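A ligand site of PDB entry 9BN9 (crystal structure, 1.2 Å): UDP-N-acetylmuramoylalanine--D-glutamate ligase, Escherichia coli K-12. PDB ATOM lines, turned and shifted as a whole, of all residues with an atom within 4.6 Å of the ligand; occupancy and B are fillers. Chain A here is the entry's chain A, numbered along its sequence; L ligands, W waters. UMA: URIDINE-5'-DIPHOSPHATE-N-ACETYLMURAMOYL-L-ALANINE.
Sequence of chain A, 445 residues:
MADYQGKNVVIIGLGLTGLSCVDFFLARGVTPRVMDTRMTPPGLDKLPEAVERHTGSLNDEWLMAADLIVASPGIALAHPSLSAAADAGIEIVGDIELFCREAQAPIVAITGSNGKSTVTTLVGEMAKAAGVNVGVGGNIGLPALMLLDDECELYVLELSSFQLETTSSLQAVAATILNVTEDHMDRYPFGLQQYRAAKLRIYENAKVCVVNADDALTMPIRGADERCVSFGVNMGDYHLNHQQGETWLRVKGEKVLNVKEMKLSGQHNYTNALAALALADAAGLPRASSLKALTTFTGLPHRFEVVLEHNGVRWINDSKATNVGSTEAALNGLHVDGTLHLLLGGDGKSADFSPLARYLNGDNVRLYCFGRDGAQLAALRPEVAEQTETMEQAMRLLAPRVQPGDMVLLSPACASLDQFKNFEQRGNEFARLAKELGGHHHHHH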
ATOM      1  N   ILE A  12      -3.899   6.076  21.101  1.00  0.00           N
ATOM      2  CA  ILE A  12      -2.480   5.899  20.873  1.00  0.00           C
ATOM      3  C   ILE A  12      -1.724   6.675  21.943  1.00  0.00           C
ATOM      4  O   ILE A  12      -1.892   7.890  22.070  1.00  0.00           O
ATOM      5  CB  ILE A  12      -2.023   6.371  19.487  1.00  0.00           C
ATOM      6  CG1 ILE A  12      -2.832   5.721  18.369  1.00  0.00           C
ATOM      7  CG2 ILE A  12      -0.527   6.090  19.331  1.00  0.00           C
ATOM      8  CD1 ILE A  12      -2.571   6.314  17.005  1.00  0.00           C
ATOM      9  N   GLY A  13      -0.881   5.951  22.672  1.00  0.00           N
ATOM     10  CA  GLY A  13      -0.042   6.504  23.711  1.00  0.00           C
ATOM     11  C   GLY A  13      -0.431   6.011  25.081  1.00  0.00           C
ATOM     12  O   GLY A  13      -1.592   6.147  25.494  1.00  0.00           O
ATOM     13  N   GLY A  15       1.146   7.031  27.907  1.00  0.00           N
ATOM     14  CA  GLY A  15       1.693   7.979  28.839  1.00  0.00           C
ATOM     15  C   GLY A  15       0.613   8.676  29.623  1.00  0.00           C
ATOM     16  O   GLY A  15      -0.497   8.167  29.800  1.00  0.00           O
ATOM     17  N   LEU A  16       0.942   9.872  30.112  1.00  0.00           N
ATOM     18  CA  LEU A  16      -0.024  10.602  30.935  1.00  0.00           C
ATOM     19  C   LEU A  16      -1.306  10.887  30.184  1.00  0.00           C
ATOM     20  O   LEU A  16      -2.412  10.728  30.718  1.00  0.00           O
ATOM     21  CB  LEU A  16       0.571  11.931  31.401  1.00  0.00           C
ATOM     22  CG  LEU A  16       1.833  11.882  32.242  1.00  0.00           C
ATOM     23  CD1 LEU A  16       2.329  13.301  32.482  1.00  0.00           C
ATOM     24  CD2 LEU A  16       1.554  11.163  33.538  1.00  0.00           C
ATOM     25  N   THR A  17      -1.184  11.323  28.925  1.00  0.00           N
ATOM     26  CA  THR A  17      -2.365  11.657  28.144  1.00  0.00           C
ATOM     27  C   THR A  17      -3.220  10.426  27.926  1.00  0.00           C
ATOM     28  O   THR A  17      -4.437  10.446  28.109  1.00  0.00           O
ATOM     29  CB  THR A  17      -1.973  12.263  26.801  1.00  0.00           C
ATOM     30  OG1 THR A  17      -1.240  13.470  27.030  1.00  0.00           O
ATOM     31  CG2 THR A  17      -3.185  12.593  25.987  1.00  0.00           C
ATOM     32  N   GLY A  18      -2.598   9.341  27.476  1.00  0.00           N
ATOM     33  CA  GLY A  18      -3.342   8.147  27.160  1.00  0.00           C
ATOM     34  C   GLY A  18      -4.108   7.623  28.365  1.00  0.00           C
ATOM     35  O   GLY A  18      -5.259   7.213  28.246  1.00  0.00           O
ATOM     36  N   ASP A  36       0.799   1.663  21.760  1.00  0.00           N
ATOM     37  CA  ASP A  36       1.948   2.567  21.859  1.00  0.00           C
ATOM     38  C   ASP A  36       3.093   1.913  21.106  1.00  0.00           C
ATOM     39  O   ASP A  36       3.271   0.701  21.193  1.00  0.00           O
ATOM     40  CB  ASP A  36       2.329   2.758  23.328  1.00  0.00           C
ATOM     41  CG  ASP A  36       3.238   3.964  23.581  1.00  0.00           C
ATOM     42  OD1 ASP A  36       4.379   3.994  23.064  1.00  0.00           O
ATOM     43  OD2 ASP A  36       2.798   4.882  24.312  1.00  0.00           O
ATOM     44  N   THR A  37       3.883   2.701  20.371  1.00  0.00           N
ATOM     45  CA  THR A  37       5.026   2.117  19.659  1.00  0.00           C
ATOM     46  C   THR A  37       6.143   1.683  20.604  1.00  0.00           C
ATOM     47  O   THR A  37       6.948   0.831  20.226  1.00  0.00           O
ATOM     48  CB  THR A  37       5.627   3.046  18.588  1.00  0.00           C
ATOM     49  OG1 THR A  37       6.215   4.187  19.206  1.00  0.00           O
ATOM     50  CG2 THR A  37       4.611   3.483  17.568  1.00  0.00           C
ATOM     51  N   ARG A  38       6.210   2.262  21.804  1.00  0.00           N
ATOM     52  CA  ARG A  38       7.209   1.837  22.778  1.00  0.00           C
ATOM     53  C   ARG A  38       6.835   0.458  23.311  1.00  0.00           C
ATOM     54  O   ARG A  38       5.667   0.163  23.554  1.00  0.00           O
ATOM     55  CB  ARG A  38       7.254   2.825  23.942  1.00  0.00           C
ATOM     56  CG  ARG A  38       7.729   4.225  23.561  1.00  0.00           C
ATOM     57  CD  ARG A  38       7.507   5.263  24.661  1.00  0.00           C
ATOM     58  NE  ARG A  38       6.089   5.621  24.784  1.00  0.00           N
ATOM     59  CZ  ARG A  38       5.628   6.510  25.653  1.00  0.00           C
ATOM     60  NH1 ARG A  38       6.424   7.150  26.481  1.00  0.00           N
ATOM     61  NH2 ARG A  38       4.321   6.775  25.679  1.00  0.00           N
ATOM     62  N   LEU A  58       2.451   0.304  16.278  1.00  0.00           N
ATOM     63  CA  LEU A  58       1.022   0.575  16.078  1.00  0.00           C
ATOM     64  C   LEU A  58       0.356  -0.625  15.425  1.00  0.00           C
ATOM     65  O   LEU A  58       0.924  -1.289  14.559  1.00  0.00           O
ATOM     66  CB  LEU A  58       0.798   1.841  15.258  1.00  0.00           C
ATOM     67  CG  LEU A  58       1.351   3.141  15.848  1.00  0.00           C
ATOM     68  CD1 LEU A  58       0.836   4.348  15.094  1.00  0.00           C
ATOM     69  CD2 LEU A  58       1.033   3.287  17.329  1.00  0.00           C
ATOM     70  N   SER A  72      -2.374  10.677  21.350  1.00  0.00           N
ATOM     71  CA  SER A  72      -1.571  11.468  22.269  1.00  0.00           C
ATOM     72  C   SER A  72      -0.655  12.400  21.472  1.00  0.00           C
ATOM     73  O   SER A  72      -0.292  12.100  20.333  1.00  0.00           O
ATOM     74  CB  SER A  72      -0.734  10.539  23.148  1.00  0.00           C
ATOM     75  OG  SER A  72      -1.541   9.751  24.022  1.00  0.00           O
ATOM     76  N   PRO A  73      -0.227  13.518  22.073  1.00  0.00           N
ATOM     77  CA  PRO A  73       0.613  14.455  21.317  1.00  0.00           C
ATOM     78  C   PRO A  73       1.952  13.882  20.908  1.00  0.00           C
ATOM     79  O   PRO A  73       2.559  14.390  19.957  1.00  0.00           O
ATOM     80  CB  PRO A  73       0.770  15.642  22.276  1.00  0.00           C
ATOM     81  CG  PRO A  73       0.514  15.071  23.649  1.00  0.00           C
ATOM     82  CD  PRO A  73      -0.565  14.036  23.412  1.00  0.00           C
ATOM     83  N   GLY A  74       2.424  12.831  21.575  1.00  0.00           N
ATOM     84  CA  GLY A  74       3.696  12.225  21.270  1.00  0.00           C
ATOM     85  C   GLY A  74       3.752  11.324  20.056  1.00  0.00           C
ATOM     86  O   GLY A  74       4.831  10.811  19.760  1.00  0.00           O
ATOM     87  N   ILE A  75       2.641  11.063  19.371  1.00  0.00           N
ATOM     88  CA  ILE A  75       2.658  10.282  18.118  1.00  0.00           C
ATOM     89  C   ILE A  75       2.432  11.246  16.962  1.00  0.00           C
ATOM     90  O   ILE A  75       1.517  12.060  16.989  1.00  0.00           O
ATOM     91  CB  ILE A  75       1.632   9.135  18.140  1.00  0.00           C
ATOM     92  CG1 ILE A  75       1.881   8.169  16.959  1.00  0.00           C
ATOM     93  CG2 ILE A  75       0.196   9.606  18.122  1.00  0.00           C
ATOM     94  CD1 ILE A  75       3.116   7.288  17.096  1.00  0.00           C
ATOM     95  N   GLY A 138      -3.221  21.110  30.822  1.00  0.00           N
ATOM     96  CA  GLY A 138      -2.691  20.918  29.491  1.00  0.00           C
ATOM     97  C   GLY A 138      -1.231  20.531  29.509  1.00  0.00           C
ATOM     98  O   GLY A 138      -0.791  19.733  30.350  1.00  0.00           O
ATOM     99  N   ASN A 139      -0.481  21.052  28.551  1.00  0.00           N
ATOM    100  CA  ASN A 139       0.922  20.696  28.372  1.00  0.00           C
ATOM    101  C   ASN A 139       1.768  21.010  29.598  1.00  0.00           C
ATOM    102  O   ASN A 139       2.865  20.443  29.753  1.00  0.00           O
ATOM    103  CB  ASN A 139       1.459  21.399  27.132  1.00  0.00           C
ATOM    104  CG  ASN A 139       2.830  20.906  26.719  1.00  0.00           C
ATOM    105  OD1 ASN A 139       2.975  19.781  26.217  1.00  0.00           O
ATOM    106  ND2 ASN A 139       3.833  21.755  26.867  1.00  0.00           N
ATOM    107  N   ILE A 140       1.298  21.897  30.478  1.00  0.00           N
ATOM    108  CA  ILE A 140       1.977  22.198  31.737  1.00  0.00           C
ATOM    109  C   ILE A 140       2.135  20.972  32.606  1.00  0.00           C
ATOM    110  O   ILE A 140       3.005  20.955  33.481  1.00  0.00           O
ATOM    111  CB  ILE A 140       1.233  23.352  32.441  1.00  0.00           C
ATOM    112  CG1 ILE A 140       2.073  23.939  33.569  1.00  0.00           C
ATOM    113  CG2 ILE A 140      -0.123  22.881  32.963  1.00  0.00           C
ATOM    114  CD1 ILE A 140       1.544  25.261  34.059  1.00  0.00           C
ATOM    115  N   GLY A 141       1.289  19.952  32.439  1.00  0.00           N
ATOM    116  CA  GLY A 141       1.523  18.690  33.124  1.00  0.00           C
ATOM    117  C   GLY A 141       0.313  18.025  33.730  1.00  0.00           C
ATOM    118  O   GLY A 141       0.408  16.857  34.106  1.00  0.00           O
ATOM    119  N   PRO A 143      -3.137  16.664  32.752  1.00  0.00           N
ATOM    120  CA  PRO A 143      -3.918  16.436  31.531  1.00  0.00           C
ATOM    121  C   PRO A 143      -5.264  17.132  31.584  1.00  0.00           C
ATOM    122  O   PRO A 143      -5.992  17.053  32.582  1.00  0.00           O
ATOM    123  CB  PRO A 143      -4.045  14.903  31.480  1.00  0.00           C
ATOM    124  CG  PRO A 143      -2.788  14.435  32.190  1.00  0.00           C
ATOM    125  CD  PRO A 143      -2.611  15.421  33.319  1.00  0.00           C
ATOM    126  N   SER A 160       0.610  22.714  23.356  1.00  0.00           N
ATOM    127  CA  SER A 160       1.748  22.529  22.474  1.00  0.00           C
ATOM    128  C   SER A 160       1.289  22.524  21.014  1.00  0.00           C
ATOM    129  O   SER A 160       0.114  22.313  20.695  1.00  0.00           O
ATOM    130  CB  SER A 160       2.422  21.202  22.758  1.00  0.00           C
ATOM    131  OG  SER A 160       1.569  20.130  22.386  1.00  0.00           O
ATOM    132  N   PHE A 162       1.901  20.116  19.076  1.00  0.00           N
ATOM    133  CA  PHE A 162       1.407  18.761  18.842  1.00  0.00           C
ATOM    134  C   PHE A 162      -0.066  18.638  19.206  1.00  0.00           C
ATOM    135  O   PHE A 162      -0.863  18.041  18.477  1.00  0.00           O
ATOM    136  CB  PHE A 162       2.170  17.739  19.680  1.00  0.00           C
ATOM    137  CG  PHE A 162       3.666  17.697  19.450  1.00  0.00           C
ATOM    138  CD1 PHE A 162       4.234  18.026  18.224  1.00  0.00           C
ATOM    139  CD2 PHE A 162       4.513  17.285  20.483  1.00  0.00           C
ATOM    140  CE1 PHE A 162       5.621  17.969  18.070  1.00  0.00           C
ATOM    141  CE2 PHE A 162       5.869  17.218  20.304  1.00  0.00           C
ATOM    142  CZ  PHE A 162       6.423  17.575  19.118  1.00  0.00           C
ATOM    143  N   GLN A 163      -0.442  19.179  20.370  1.00  0.00           N
ATOM    144  CA  GLN A 163      -1.847  19.137  20.776  1.00  0.00           C
ATOM    145  C   GLN A 163      -2.726  19.908  19.797  1.00  0.00           C
ATOM    146  O   GLN A 163      -3.833  19.476  19.463  1.00  0.00           O
ATOM    147  CB  GLN A 163      -2.013  19.725  22.180  1.00  0.00           C
ATOM    148  CG  GLN A 163      -1.433  18.855  23.255  1.00  0.00           C
ATOM    149  CD  GLN A 163      -1.263  19.557  24.595  1.00  0.00           C
ATOM    150  OE1 GLN A 163      -0.973  20.737  24.673  1.00  0.00           O
ATOM    151  NE2 GLN A 163      -1.426  18.818  25.667  1.00  0.00           N
ATOM    152  N   ASP A 183      12.016  24.520  17.342  1.00  0.00           N
ATOM    153  CA  ASP A 183      11.863  23.425  18.291  1.00  0.00           C
ATOM    154  C   ASP A 183      11.152  22.303  17.558  1.00  0.00           C
ATOM    155  O   ASP A 183      10.487  22.518  16.538  1.00  0.00           O
ATOM    156  CB  ASP A 183      11.056  23.878  19.525  1.00  0.00           C
ATOM    157  CG  ASP A 183      11.228  22.957  20.748  1.00  0.00           C
ATOM    158  OD1 ASP A 183      11.968  21.958  20.684  1.00  0.00           O
ATOM    159  OD2 ASP A 183      10.625  23.291  21.794  1.00  0.00           O
ATOM    160  N   HIS A 184      11.290  21.088  18.073  1.00  0.00           N
ATOM    161  CA  HIS A 184      10.537  19.926  17.578  1.00  0.00           C
ATOM    162  C   HIS A 184      10.776  19.661  16.101  1.00  0.00           C
ATOM    163  O   HIS A 184       9.898  19.127  15.415  1.00  0.00           O
ATOM    164  CB  HIS A 184       9.052  20.061  17.899  1.00  0.00           C
ATOM    165  CG  HIS A 184       8.814  20.116  19.367  1.00  0.00           C
ATOM    166  ND1 HIS A 184       9.253  19.118  20.209  1.00  0.00           N
ATOM    167  CD2 HIS A 184       8.259  21.069  20.152  1.00  0.00           C
ATOM    168  CE1 HIS A 184       8.953  19.453  21.456  1.00  0.00           C
ATOM    169  NE2 HIS A 184       8.347  20.616  21.450  1.00  0.00           N
ATOM    170  N   LEU A 417      14.568  13.211  27.269  1.00  0.00           N
ATOM    171  CA  LEU A 417      14.029  11.862  27.163  1.00  0.00           C
ATOM    172  C   LEU A 417      15.070  10.813  26.830  1.00  0.00           C
ATOM    173  O   LEU A 417      14.788   9.623  26.980  1.00  0.00           O
ATOM    174  CB  LEU A 417      12.923  11.798  26.110  1.00  0.00           C
ATOM    175  CG  LEU A 417      13.348  11.748  24.632  1.00  0.00           C
ATOM    176  CD1 LEU A 417      12.249  11.193  23.729  1.00  0.00           C
ATOM    177  CD2 LEU A 417      13.761  13.148  24.177  1.00  0.00           C
ATOM    178  N   PHE A 423      11.762  16.232  32.304  1.00  0.00           N
ATOM    179  CA  PHE A 423      12.666  17.323  32.655  1.00  0.00           C
ATOM    180  C   PHE A 423      12.661  17.589  34.146  1.00  0.00           C
ATOM    181  O   PHE A 423      13.651  18.096  34.687  1.00  0.00           O
ATOM    182  CB  PHE A 423      12.375  18.600  31.842  1.00  0.00           C
ATOM    183  CG  PHE A 423      11.101  19.297  32.237  1.00  0.00           C
ATOM    184  CD1 PHE A 423      11.033  20.054  33.392  1.00  0.00           C
ATOM    185  CD2 PHE A 423       9.978  19.191  31.450  1.00  0.00           C
ATOM    186  CE1 PHE A 423       9.859  20.688  33.759  1.00  0.00           C
ATOM    187  CE2 PHE A 423       8.804  19.833  31.810  1.00  0.00           C
ATOM    188  CZ  PHE A 423       8.752  20.573  32.964  1.00  0.00           C
HETATM  189  N1  UMA L   1       5.788   7.993  22.116  1.00  0.00           N
HETATM  190  C2  UMA L   1       6.195   6.968  21.294  1.00  0.00           C
HETATM  191  N3  UMA L   1       5.174   6.201  20.790  1.00  0.00           N
HETATM  192  C4  UMA L   1       3.822   6.343  21.016  1.00  0.00           C
HETATM  193  C5  UMA L   1       3.476   7.437  21.881  1.00  0.00           C
HETATM  194  C6  UMA L   1       4.452   8.204  22.396  1.00  0.00           C
HETATM  195  O2  UMA L   1       7.364   6.757  21.032  1.00  0.00           O
HETATM  196  O4  UMA L   1       3.045   5.531  20.525  1.00  0.00           O
HETATM  197  C1B UMA L   1       6.804   8.876  22.704  1.00  0.00           C
HETATM  198  C2B UMA L   1       6.648  10.319  22.216  1.00  0.00           C
HETATM  199  O2' UMA L   1       7.245  10.566  20.968  1.00  0.00           O
HETATM  200  C3B UMA L   1       7.324  11.051  23.378  1.00  0.00           C
HETATM  201  C4B UMA L   1       6.824  10.261  24.591  1.00  0.00           C
HETATM  202  O4B UMA L   1       6.534   8.930  24.085  1.00  0.00           O
HETATM  203  O3B UMA L   1       8.743  10.960  23.276  1.00  0.00           O
HETATM  204  C5B UMA L   1       5.636  10.794  25.348  1.00  0.00           C
HETATM  205  O5B UMA L   1       4.513  10.983  24.471  1.00  0.00           O
HETATM  206  PA  UMA L   1       3.050  11.022  25.121  1.00  0.00           P
HETATM  207  O1A UMA L   1       2.733   9.730  25.771  1.00  0.00           O
HETATM  208  O2A UMA L   1       2.113  11.585  24.089  1.00  0.00           O
HETATM  209  O3A UMA L   1       3.284  12.087  26.273  1.00  0.00           O
HETATM  210  PB  UMA L   1       2.517  12.265  27.675  1.00  0.00           P
HETATM  211  O1B UMA L   1       3.199  11.487  28.747  1.00  0.00           O
HETATM  212  O2B UMA L   1       1.063  12.046  27.485  1.00  0.00           O
HETATM  213  O1' UMA L   1       2.811  13.813  27.917  1.00  0.00           O
HETATM  214  C1' UMA L   1       2.176  14.760  27.069  1.00  0.00           C
HETATM  215  C2' UMA L   1       3.172  15.892  26.780  1.00  0.00           C
HETATM  216  N2' UMA L   1       4.313  15.386  26.047  1.00  0.00           N
HETATM  217  C7' UMA L   1       4.466  15.552  24.734  1.00  0.00           C
HETATM  218  O7' UMA L   1       3.670  16.175  24.036  1.00  0.00           O
HETATM  219  C8' UMA L   1       5.671  14.877  24.148  1.00  0.00           C
HETATM  220  C3' UMA L   1       3.497  16.582  28.090  1.00  0.00           C
HETATM  221  O3' UMA L   1       4.341  17.713  27.875  1.00  0.00           O
HETATM  222  C4' UMA L   1       2.200  17.099  28.699  1.00  0.00           C
HETATM  223  O4' UMA L   1       2.444  17.683  29.970  1.00  0.00           O
HETATM  224  C5' UMA L   1       1.193  15.987  28.894  1.00  0.00           C
HETATM  225  O5' UMA L   1       0.989  15.252  27.674  1.00  0.00           O
HETATM  226  C6' UMA L   1      -0.183  16.481  29.295  1.00  0.00           C
HETATM  227  O6' UMA L   1      -0.785  17.314  28.295  1.00  0.00           O
HETATM  228  C18 UMA L   1       5.737  17.427  28.001  1.00  0.00           C
HETATM  229  C19 UMA L   1       6.476  17.890  26.762  1.00  0.00           C
HETATM  230  O18 UMA L   1       7.667  17.625  26.632  1.00  0.00           O
HETATM  231  C20 UMA L   1       6.265  18.176  29.198  1.00  0.00           C
HETATM  232  N4  UMA L   1       5.785  18.588  25.864  1.00  0.00           N
HETATM  233  C21 UMA L   1       6.430  19.155  24.693  1.00  0.00           C
HETATM  234  C22 UMA L   1       7.048  20.520  25.014  1.00  0.00           C
HETATM  235  O19 UMA L   1       7.887  20.931  24.207  1.00  0.00           O
HETATM  236  O20 UMA L   1       6.694  21.100  26.049  1.00  0.00           O
HETATM  237  C23 UMA L   1       5.437  19.272  23.558  1.00  0.00           C
HETATM  238  O   HOH W   1       7.837  23.593  26.022  1.00  0.00           O
HETATM  239  O   HOH W   2       1.833  18.234  24.258  1.00  0.00           O
HETATM  240  O   HOH W   3       4.030  16.389  31.907  1.00  0.00           O
HETATM  241  O   HOH W   4       5.434  12.734  29.792  1.00  0.00           O
HETATM  242  O   HOH W   5       4.142   9.140  30.961  1.00  0.00           O
HETATM  243  O   HOH W   6      10.209   8.734  23.988  1.00  0.00           O
HETATM  244  O   HOH W   7       6.411  13.896  27.475  1.00  0.00           O
HETATM  245  O   HOH W   8       8.686  12.842  26.021  1.00  0.00           O
HETATM  246  O   HOH W   9      10.478  21.932  24.138  1.00  0.00           O
HETATM  247  O   HOH W  10       8.946  15.443  26.717  1.00  0.00           O
HETATM  248  O   HOH W  11       4.950   9.159  28.439  1.00  0.00           O
HETATM  249  O   HOH W  12       0.031   9.066  26.260  1.00  0.00           O
HETATM  250  O   HOH W  13      -3.605  17.824  28.357  1.00  0.00           O
HETATM  251  O   HOH W  14      -1.855  15.949  25.945  1.00  0.00           O
HETATM  252  O   HOH W  15       5.396  20.990  30.860  1.00  0.00           O
HETATM  253  O   HOH W  16       9.939  10.441  20.113  1.00  0.00           O
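The side-chain amide nitrogen (NE2) of Gln 163 is in hydrogen-bond range of an oxygen (O6') of the ligand (3.1 Å). OD1 of Asp 36 sits close to N3 of the ligand. N3 of the ligand lies within hydrogen-bond range of OG1 of Thr 37, at 2.8 Å. O of Gly 74 is in hydrogen-bond range of O2' of the ligand (2.7 Å). The backbone carbonyl oxygen (O) of Gly 138 lies within hydrogen-bond range of an oxygen (O6') of the ligand, at 3.2 Å. The backbone NH of Leu 16 lies within hydrogen-bond range of an oxygen (O1B) of the ligand (3.1 Å). An oxygen (O19) of the ligand sits at hydrogen-bond distance from a ring nitrogen (NE2) of His 184, 2.8 Å away. The side-chain amide oxygen of Asn 139 sits close to an oxygen (O3') of the ligand (3.0 Å). The backbone carbonyl oxygen of Asn 139 is in hydrogen-bond range of an oxygen (O4') of the ligand, 2.8 Å away. An oxygen (O2A) of the ligand lies within hydrogen-bond range of the backbone NH of Gly 74, at 2.8 Å. N of Thr 37 is in hydrogen-bond range of O4 of the ligand (3.0 Å). The side-chain hydroxyl (OG1) of Thr 17 lies within hydrogen-bond range of an oxygen (O2B) of the ligand. The guanidinium group of Arg 38 lies within salt-bridge range of an oxygen (O1A) of the ligand (3.4 Å). The backbone NH (N) of Thr 17 is in hydrogen-bond range of an oxygen (O2B) of the ligand, at 2.8 Å.
Ile 12 touches the ligand. Gly 15 touches the ligand (CA to O1A, 3.7 Å). Ser 72 touches the ligand (CB to O2A, 3.2 Å). Pro 73 touches the ligand. Ile 75 touches the ligand. CA of Gly 141 touches O4' of the ligand (3.4 Å). Ser 160 touches the ligand (CB to C23, 3.7 Å). Phe 162 touches the ligand (CD2 to C23, 3.8 Å). Leu 417 touches the ligand. Of the 26 residues printed, 19 come within 4 Å of the ligand. Along chain A the residues within 4 Å of the ligand span positions 12 to 417. The nearest printed residue that does not touch the ligand is Phe 423 (4.002 Å).
Water W2 lies within hydrogen-bond range of the side-chain hydroxyl of Ser 160 (2.7 Å), the side-chain amide oxygen of Asn 139 (2.7 Å) and an oxygen (O7') of the ligand (2.8 Å). Water W9 lies within hydrogen-bond range of the side-chain carboxylate of Asp 183 (2.7 Å) and an oxygen (O19) of the ligand (2.8 Å). Water W12 lies within hydrogen-bond range of OG of Ser 72, O1A of the ligand, N of Gly 15, N of Gly 18 and O of Gly 13. Water W14 lies within hydrogen-bond range of the side-chain hydroxyl (OG1) of Thr 17, the side-chain amide nitrogen (NE2) of Gln 163 and an oxygen (O6') of the ligand. Water W11 bridges an oxygen (O1B) of the ligand (2.9 Å) and the guanidinium group (NH1) of Arg 38 (3.2 Å). Water W5 bridges O1B of the ligand (3.4 Å) and N of Leu 16 (3.4 Å).
The side-chain hydroxyl (OG) of Ser 160 lies close to the backbone NH (N) of Phe 162. The guanidinium group of Arg 38 lies within salt-bridge range of the side-chain carboxylate of Asp 36 (2.8 Å). OG of Ser 72 is in hydrogen-bond range of O of Ile 12 (2.7 Å). The side-chain amide oxygen (OE1) of Gln 163 is in hydrogen-bond range of the backbone NH (N) of Ser 160, at 2.9 Å.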
